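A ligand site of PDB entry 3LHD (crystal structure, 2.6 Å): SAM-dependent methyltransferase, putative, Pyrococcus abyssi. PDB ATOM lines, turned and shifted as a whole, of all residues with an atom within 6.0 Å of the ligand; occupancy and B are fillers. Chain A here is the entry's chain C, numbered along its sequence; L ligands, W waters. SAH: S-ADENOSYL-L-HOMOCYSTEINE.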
ATOM      1  N   GLN A  75      15.177  -0.691   4.233  1.00  0.00           N
ATOM      2  CA  GLN A  75      14.224  -1.808   4.168  1.00  0.00           C
ATOM      3  C   GLN A  75      14.292  -2.595   2.839  1.00  0.00           C
ATOM      4  O   GLN A  75      15.373  -2.842   2.310  1.00  0.00           O
ATOM      5  CB  GLN A  75      12.789  -1.358   4.497  1.00  0.00           C
ATOM      6  CG  GLN A  75      12.135  -0.411   3.489  1.00  0.00           C
ATOM      7  CD  GLN A  75      12.347   1.048   3.836  1.00  0.00           C
ATOM      8  OE1 GLN A  75      13.477   1.516   4.015  1.00  0.00           O
ATOM      9  NE2 GLN A  75      11.239   1.801   3.937  1.00  0.00           N
ATOM     10  N   ALA A 100      14.513  -2.857 -11.619  1.00  0.00           N
ATOM     11  CA  ALA A 100      15.521  -1.897 -11.194  1.00  0.00           C
ATOM     12  C   ALA A 100      15.289  -1.480  -9.760  1.00  0.00           C
ATOM     13  O   ALA A 100      14.179  -1.111  -9.347  1.00  0.00           O
ATOM     14  CB  ALA A 100      15.569  -0.699 -12.093  1.00  0.00           C
ATOM     15  N   GLY A 101      16.395  -1.498  -9.029  1.00  0.00           N
ATOM     16  CA  GLY A 101      16.407  -1.401  -7.617  1.00  0.00           C
ATOM     17  C   GLY A 101      16.535  -2.823  -7.155  1.00  0.00           C
ATOM     18  O   GLY A 101      15.546  -3.416  -6.724  1.00  0.00           O
ATOM     19  N   VAL A 102      17.729  -3.404  -7.275  1.00  0.00           N
ATOM     20  CA  VAL A 102      17.951  -4.743  -6.775  1.00  0.00           C
ATOM     21  C   VAL A 102      18.033  -4.799  -5.253  1.00  0.00           C
ATOM     22  O   VAL A 102      17.705  -5.809  -4.649  1.00  0.00           O
ATOM     23  CB  VAL A 102      19.162  -5.459  -7.429  1.00  0.00           C
ATOM     24  CG1 VAL A 102      20.469  -4.972  -6.835  1.00  0.00           C
ATOM     25  CG2 VAL A 102      19.036  -6.991  -7.260  1.00  0.00           C
ATOM     26  N   GLY A 103      18.484  -3.696  -4.640  1.00  0.00           N
ATOM     27  CA  GLY A 103      18.661  -3.624  -3.183  1.00  0.00           C
ATOM     28  C   GLY A 103      19.352  -4.868  -2.645  1.00  0.00           C
ATOM     29  O   GLY A 103      20.366  -5.306  -3.181  1.00  0.00           O
ATOM     30  N   SER A 104      18.791  -5.438  -1.581  1.00  0.00           N
ATOM     31  CA  SER A 104      19.303  -6.676  -0.992  1.00  0.00           C
ATOM     32  C   SER A 104      19.020  -7.906  -1.847  1.00  0.00           C
ATOM     33  O   SER A 104      19.611  -8.959  -1.625  1.00  0.00           O
ATOM     34  CB  SER A 104      18.692  -6.882   0.381  1.00  0.00           C
ATOM     35  OG  SER A 104      19.356  -6.080   1.325  1.00  0.00           O
ATOM     36  N   TYR A 124      18.757  -4.258 -12.477  1.00  0.00           N
ATOM     37  CA  TYR A 124      19.650  -3.111 -12.587  1.00  0.00           C
ATOM     38  C   TYR A 124      19.955  -2.572 -11.202  1.00  0.00           C
ATOM     39  O   TYR A 124      19.113  -2.617 -10.318  1.00  0.00           O
ATOM     40  CB  TYR A 124      19.021  -2.019 -13.446  1.00  0.00           C
ATOM     41  CG  TYR A 124      19.018  -2.266 -14.938  1.00  0.00           C
ATOM     42  CD1 TYR A 124      19.752  -1.453 -15.800  1.00  0.00           C
ATOM     43  CD2 TYR A 124      18.267  -3.299 -15.496  1.00  0.00           C
ATOM     44  CE1 TYR A 124      19.747  -1.666 -17.169  1.00  0.00           C
ATOM     45  CE2 TYR A 124      18.257  -3.525 -16.863  1.00  0.00           C
ATOM     46  CZ  TYR A 124      19.005  -2.703 -17.699  1.00  0.00           C
ATOM     47  OH  TYR A 124      18.995  -2.912 -19.056  1.00  0.00           O
ATOM     48  N   GLU A 125      21.176  -2.077 -11.031  1.00  0.00           N
ATOM     49  CA  GLU A 125      21.618  -1.490  -9.770  1.00  0.00           C
ATOM     50  C   GLU A 125      22.688  -0.448 -10.079  1.00  0.00           C
ATOM     51  O   GLU A 125      23.428  -0.590 -11.040  1.00  0.00           O
ATOM     52  CB  GLU A 125      22.143  -2.573  -8.826  1.00  0.00           C
ATOM     53  CG  GLU A 125      22.541  -2.107  -7.413  1.00  0.00           C
ATOM     54  CD  GLU A 125      21.497  -1.194  -6.742  1.00  0.00           C
ATOM     55  OE1 GLU A 125      21.833  -0.020  -6.457  1.00  0.00           O
ATOM     56  OE2 GLU A 125      20.354  -1.641  -6.489  1.00  0.00           O
ATOM     57  N   ILE A 126      22.733   0.621  -9.288  1.00  0.00           N
ATOM     58  CA  ILE A 126      23.739   1.676  -9.499  1.00  0.00           C
ATOM     59  C   ILE A 126      24.749   1.694  -8.364  1.00  0.00           C
ATOM     60  O   ILE A 126      25.837   2.261  -8.505  1.00  0.00           O
ATOM     61  CB  ILE A 126      23.119   3.090  -9.728  1.00  0.00           C
ATOM     62  CG1 ILE A 126      22.291   3.552  -8.522  1.00  0.00           C
ATOM     63  CG2 ILE A 126      22.286   3.098 -10.989  1.00  0.00           C
ATOM     64  CD1 ILE A 126      21.697   4.952  -8.666  1.00  0.00           C
ATOM     65  N   ARG A 127      24.401   1.048  -7.267  1.00  0.00           N
ATOM     66  CA  ARG A 127      25.226   1.011  -6.079  1.00  0.00           C
ATOM     67  C   ARG A 127      25.993  -0.301  -6.067  1.00  0.00           C
ATOM     68  O   ARG A 127      25.388  -1.381  -6.032  1.00  0.00           O
ATOM     69  CB  ARG A 127      24.347   1.164  -4.833  1.00  0.00           C
ATOM     70  CG  ARG A 127      25.088   1.509  -3.569  1.00  0.00           C
ATOM     71  CD  ARG A 127      24.995   2.976  -3.218  1.00  0.00           C
ATOM     72  NE  ARG A 127      23.928   3.273  -2.249  1.00  0.00           N
ATOM     73  CZ  ARG A 127      24.031   3.121  -0.924  1.00  0.00           C
ATOM     74  NH1 ARG A 127      25.123   2.631  -0.353  1.00  0.00           N
ATOM     75  NH2 ARG A 127      22.995   3.441  -0.157  1.00  0.00           N
ATOM     76  N   PHE A 130      25.468  -2.817  -2.947  1.00  0.00           N
ATOM     77  CA  PHE A 130      24.169  -3.496  -2.997  1.00  0.00           C
ATOM     78  C   PHE A 130      24.154  -4.620  -4.035  1.00  0.00           C
ATOM     79  O   PHE A 130      23.546  -5.673  -3.805  1.00  0.00           O
ATOM     80  CB  PHE A 130      23.020  -2.535  -3.283  1.00  0.00           C
ATOM     81  CG  PHE A 130      22.719  -1.573  -2.163  1.00  0.00           C
ATOM     82  CD1 PHE A 130      22.085  -0.349  -2.444  1.00  0.00           C
ATOM     83  CD2 PHE A 130      23.044  -1.872  -0.841  1.00  0.00           C
ATOM     84  CE1 PHE A 130      21.782   0.555  -1.424  1.00  0.00           C
ATOM     85  CE2 PHE A 130      22.758  -0.973   0.187  1.00  0.00           C
ATOM     86  CZ  PHE A 130      22.129   0.247  -0.106  1.00  0.00           C
ATOM     87  N   LYS A 152      24.280  -0.956 -13.656  1.00  0.00           N
ATOM     88  CA  LYS A 152      23.922  -0.021 -14.701  1.00  0.00           C
ATOM     89  C   LYS A 152      22.672   0.784 -14.306  1.00  0.00           C
ATOM     90  O   LYS A 152      21.737   0.248 -13.693  1.00  0.00           O
ATOM     91  CB  LYS A 152      23.722  -0.792 -16.000  1.00  0.00           C
ATOM     92  CG  LYS A 152      23.496   0.036 -17.222  1.00  0.00           C
ATOM     93  CD  LYS A 152      23.194  -0.851 -18.439  1.00  0.00           C
ATOM     94  CE  LYS A 152      24.451  -1.123 -19.267  1.00  0.00           C
ATOM     95  NZ  LYS A 152      24.149  -1.085 -20.737  1.00  0.00           N
ATOM     96  N   ASP A 153      22.679   2.069 -14.648  1.00  0.00           N
ATOM     97  CA  ASP A 153      21.605   3.017 -14.363  1.00  0.00           C
ATOM     98  C   ASP A 153      20.481   2.860 -15.374  1.00  0.00           C
ATOM     99  O   ASP A 153      20.591   3.332 -16.492  1.00  0.00           O
ATOM    100  CB  ASP A 153      22.163   4.455 -14.443  1.00  0.00           C
ATOM    101  CG  ASP A 153      21.197   5.498 -13.897  1.00  0.00           C
ATOM    102  OD1 ASP A 153      21.680   6.500 -13.310  1.00  0.00           O
ATOM    103  OD2 ASP A 153      19.974   5.356 -14.063  1.00  0.00           O
ATOM    104  N   ILE A 154      19.402   2.212 -14.950  1.00  0.00           N
ATOM    105  CA  ILE A 154      18.252   1.960 -15.834  1.00  0.00           C
ATOM    106  C   ILE A 154      17.665   3.232 -16.462  1.00  0.00           C
ATOM    107  O   ILE A 154      16.984   3.145 -17.491  1.00  0.00           O
ATOM    108  CB  ILE A 154      17.136   1.150 -15.122  1.00  0.00           C
ATOM    109  CG1 ILE A 154      16.358   0.297 -16.140  1.00  0.00           C
ATOM    110  CG2 ILE A 154      16.223   2.068 -14.317  1.00  0.00           C
ATOM    111  CD1 ILE A 154      15.288  -0.585 -15.545  1.00  0.00           C
ATOM    112  N   TYR A 155      17.911   4.397 -15.859  1.00  0.00           N
ATOM    113  CA  TYR A 155      17.403   5.673 -16.412  1.00  0.00           C
ATOM    114  C   TYR A 155      17.974   5.965 -17.797  1.00  0.00           C
ATOM    115  O   TYR A 155      17.302   6.573 -18.633  1.00  0.00           O
ATOM    116  CB  TYR A 155      17.648   6.875 -15.490  1.00  0.00           C
ATOM    117  CG  TYR A 155      16.945   6.826 -14.149  1.00  0.00           C
ATOM    118  CD1 TYR A 155      17.484   7.476 -13.040  1.00  0.00           C
ATOM    119  CD2 TYR A 155      15.750   6.132 -13.989  1.00  0.00           C
ATOM    120  CE1 TYR A 155      16.841   7.420 -11.810  1.00  0.00           C
ATOM    121  CE2 TYR A 155      15.098   6.078 -12.763  1.00  0.00           C
ATOM    122  CZ  TYR A 155      15.646   6.720 -11.680  1.00  0.00           C
ATOM    123  OH  TYR A 155      14.999   6.653 -10.471  1.00  0.00           O
ATOM    124  N   ASP A 169      11.238  -0.252  -8.209  1.00  0.00           N
ATOM    125  CA  ASP A 169      11.044   0.296  -6.885  1.00  0.00           C
ATOM    126  C   ASP A 169      12.077   1.404  -6.581  1.00  0.00           C
ATOM    127  O   ASP A 169      12.448   1.612  -5.423  1.00  0.00           O
ATOM    128  CB  ASP A 169      11.070  -0.827  -5.834  1.00  0.00           C
ATOM    129  CG  ASP A 169      12.458  -1.311  -5.536  1.00  0.00           C
ATOM    130  OD1 ASP A 169      12.590  -2.018  -4.510  1.00  0.00           O
ATOM    131  OD2 ASP A 169      13.403  -0.967  -6.279  1.00  0.00           O
ATOM    132  N   LEU A 170      12.523   2.097  -7.619  1.00  0.00           N
ATOM    133  CA  LEU A 170      13.501   3.186  -7.503  1.00  0.00           C
ATOM    134  C   LEU A 170      12.829   4.552  -7.324  1.00  0.00           C
ATOM    135  O   LEU A 170      11.616   4.648  -7.504  1.00  0.00           O
ATOM    136  CB  LEU A 170      14.443   3.201  -8.720  1.00  0.00           C
ATOM    137  CG  LEU A 170      13.901   2.787 -10.085  1.00  0.00           C
ATOM    138  CD1 LEU A 170      12.995   3.853 -10.697  1.00  0.00           C
ATOM    139  CD2 LEU A 170      15.064   2.501 -10.990  1.00  0.00           C
ATOM    140  N   PRO A 171      13.602   5.609  -6.973  1.00  0.00           N
ATOM    141  CA  PRO A 171      12.954   6.900  -6.640  1.00  0.00           C
ATOM    142  C   PRO A 171      12.103   7.512  -7.749  1.00  0.00           C
ATOM    143  O   PRO A 171      11.032   8.041  -7.455  1.00  0.00           O
ATOM    144  CB  PRO A 171      14.133   7.813  -6.295  1.00  0.00           C
ATOM    145  CG  PRO A 171      15.244   6.866  -5.869  1.00  0.00           C
ATOM    146  CD  PRO A 171      15.066   5.671  -6.785  1.00  0.00           C
ATOM    147  N   TYR A 193       6.686   0.546  -7.527  1.00  0.00           N
ATOM    148  CA  TYR A 193       6.470   0.657  -6.102  1.00  0.00           C
ATOM    149  C   TYR A 193       7.018   2.005  -5.616  1.00  0.00           C
ATOM    150  O   TYR A 193       8.186   2.324  -5.824  1.00  0.00           O
ATOM    151  CB  TYR A 193       7.155  -0.506  -5.380  1.00  0.00           C
ATOM    152  CG  TYR A 193       7.210  -0.390  -3.879  1.00  0.00           C
ATOM    153  CD1 TYR A 193       8.290   0.245  -3.246  1.00  0.00           C
ATOM    154  CD2 TYR A 193       6.215  -0.944  -3.092  1.00  0.00           C
ATOM    155  CE1 TYR A 193       8.352   0.340  -1.870  1.00  0.00           C
ATOM    156  CE2 TYR A 193       6.272  -0.854  -1.708  1.00  0.00           C
ATOM    157  CZ  TYR A 193       7.343  -0.214  -1.104  1.00  0.00           C
ATOM    158  OH  TYR A 193       7.419  -0.125   0.263  1.00  0.00           O
ATOM    159  N   PRO A 195       6.793   4.683  -2.126  1.00  0.00           N
ATOM    160  CA  PRO A 195       6.285   5.029  -0.793  1.00  0.00           C
ATOM    161  C   PRO A 195       5.440   6.318  -0.723  1.00  0.00           C
ATOM    162  O   PRO A 195       4.496   6.347   0.051  1.00  0.00           O
ATOM    163  CB  PRO A 195       7.568   5.185   0.039  1.00  0.00           C
ATOM    164  CG  PRO A 195       8.583   4.379  -0.680  1.00  0.00           C
ATOM    165  CD  PRO A 195       8.251   4.508  -2.129  1.00  0.00           C
ATOM    166  N   CYS A 196       5.762   7.338  -1.506  1.00  0.00           N
ATOM    167  CA  CYS A 196       5.108   8.658  -1.368  1.00  0.00           C
ATOM    168  C   CYS A 196       3.986   8.919  -2.347  1.00  0.00           C
ATOM    169  O   CYS A 196       4.029   8.471  -3.484  1.00  0.00           O
ATOM    170  CB  CYS A 196       6.122   9.810  -1.467  1.00  0.00           C
ATOM    171  SG  CYS A 196       7.593   9.665  -0.446  1.00  0.00           S
ATOM    172  N   GLN A 199       5.458  10.709  -5.597  1.00  0.00           N
ATOM    173  CA  GLN A 199       5.967   9.777  -6.587  1.00  0.00           C
ATOM    174  C   GLN A 199       4.861   9.224  -7.487  1.00  0.00           C
ATOM    175  O   GLN A 199       5.047   9.145  -8.705  1.00  0.00           O
ATOM    176  CB  GLN A 199       6.732   8.655  -5.897  1.00  0.00           C
ATOM    177  CG  GLN A 199       8.025   9.115  -5.236  1.00  0.00           C
ATOM    178  CD  GLN A 199       8.709   8.018  -4.450  1.00  0.00           C
ATOM    179  OE1 GLN A 199       8.153   7.479  -3.482  1.00  0.00           O
ATOM    180  NE2 GLN A 199       9.944   7.694  -4.841  1.00  0.00           N
HETATM  181  N   SAH L   1      12.526   3.288  -0.608  1.00  0.00           N
HETATM  182  CA  SAH L   1      13.402   4.285  -1.306  1.00  0.00           C
HETATM  183  CB  SAH L   1      13.988   3.650  -2.574  1.00  0.00           C
HETATM  184  CG  SAH L   1      15.455   3.232  -2.412  1.00  0.00           C
HETATM  185  SD  SAH L   1      16.214   3.019  -3.998  1.00  0.00           S
HETATM  186  C   SAH L   1      12.581   5.524  -1.613  1.00  0.00           C
HETATM  187  O   SAH L   1      11.880   6.053  -0.747  1.00  0.00           O
HETATM  188  OXT SAH L   1      12.580   6.051  -2.728  1.00  0.00           O
HETATM  189  C5' SAH L   1      16.063   1.271  -4.240  1.00  0.00           C
HETATM  190  C4' SAH L   1      17.253   0.645  -4.972  1.00  0.00           C
HETATM  191  O4' SAH L   1      17.318   1.047  -6.352  1.00  0.00           O
HETATM  192  C3' SAH L   1      18.600   1.009  -4.385  1.00  0.00           C
HETATM  193  O3' SAH L   1      19.349  -0.204  -4.327  1.00  0.00           O
HETATM  194  C2' SAH L   1      19.212   1.980  -5.386  1.00  0.00           C
HETATM  195  O2' SAH L   1      20.634   1.985  -5.361  1.00  0.00           O
HETATM  196  C1' SAH L   1      18.641   1.458  -6.700  1.00  0.00           C
HETATM  197  N9  SAH L   1      18.539   2.448  -7.781  1.00  0.00           N
HETATM  198  C8  SAH L   1      18.185   3.741  -7.673  1.00  0.00           C
HETATM  199  N7  SAH L   1      18.173   4.341  -8.896  1.00  0.00           N
HETATM  200  C5  SAH L   1      18.524   3.421  -9.805  1.00  0.00           C
HETATM  201  C6  SAH L   1      18.710   3.389 -11.270  1.00  0.00           C
HETATM  202  N6  SAH L   1      18.504   4.496 -12.009  1.00  0.00           N
HETATM  203  N1  SAH L   1      19.072   2.214 -11.850  1.00  0.00           N
HETATM  204  C2  SAH L   1      19.278   1.107 -11.111  1.00  0.00           C
HETATM  205  N3  SAH L   1      19.125   1.077  -9.779  1.00  0.00           N
HETATM  206  C4  SAH L   1      18.752   2.177  -9.066  1.00  0.00           C
HETATM  207  O   HOH W   1      10.929   2.944  -3.851  1.00  0.00           O
HETATM  208  O   HOH W   2      20.905   4.804  -4.736  1.00  0.00           O
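Gly 101 touches the ligand. N of Gly 103 touches O3' of the ligand, 3.6 Å away. O of Tyr 124 touches N3 of the ligand, at 3.7 Å. CG2 of Ile 126 touches N1 of the ligand, at 3.4 Å. CB of Arg 127 touches O2' of the ligand, 3.8 Å away. CD1 of Phe 130 touches O3' of the ligand, at 3.3 Å. Lys 152 touches the ligand (O to C2, 3.7 Å). Tyr 155 touches the ligand (CD1 to N6, 3.3 Å). Asp 169 touches the ligand. Leu 170 touches the ligand. Pro 171 touches the ligand (CD to C8, 3.8 Å). Pro 195 touches the ligand (CG to O, 3.7 Å). NE2 of Gln 199 touches OXT of the ligand, at 3.8 Å. Hydrophobic or aromatic side chains within 4 Å of the ligand: Tyr 124, Ile 126, Phe 130, Ile 154, Tyr 155, Leu 170, Pro 171 and Pro 195. 16 residues have an atom within 4 Å of the ligand: Gly 101, Gly 103, Tyr 124, Glu 125, Ile 126, Arg 127, Phe 130, Lys 152, Asp 153, Ile 154, Tyr 155, Asp 169, Leu 170, Pro 171, Pro 195 and Gln 199.
The side-chain carboxylate (OE1) of Glu 125 lies within hydrogen-bond range of an oxygen (O2') of the ligand (2.6 Å). OD2 of Asp 153 lies within hydrogen-bond range of N6 of the ligand, 2.7 Å away. A nitrogen (N1) of the ligand is in hydrogen-bond range of the backbone NH (N) of Ile 154, 3.1 Å away.
Water W1 bridges the backbone carbonyl oxygen of Asp 169 (2.6 Å) and the backbone carbonyl oxygen of Tyr 193 (3.4 Å).
The backbone NH (N) of Gly 103 is in hydrogen-bond range of the side-chain carboxylate (OE2) of Glu 125, 3.3 Å away. The backbone carbonyl oxygen (O) of Glu 125 is in hydrogen-bond range of the backbone NH (N) of Lys 152 (2.8 Å). The side-chain carboxylate of Glu 125 lies within hydrogen-bond range of the backbone NH of Val 102 (3.3 Å). The backbone NH of Gly 101 sits at hydrogen-bond distance from the backbone carbonyl oxygen of Tyr 124. O of Tyr 124 is in hydrogen-bond range of N of Val 102, 3.4 Å away. NE2 of Gln 199 is in hydrogen-bond range of O of Pro 171 (2.9 Å). The side-chain amide oxygen (OE1) of Gln 199 lies within hydrogen-bond range of the backbone NH (N) of Cys 196, at 3.1 Å. N of Asp 169 is in hydrogen-bond range of O of Ala 100 (3.3 Å).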
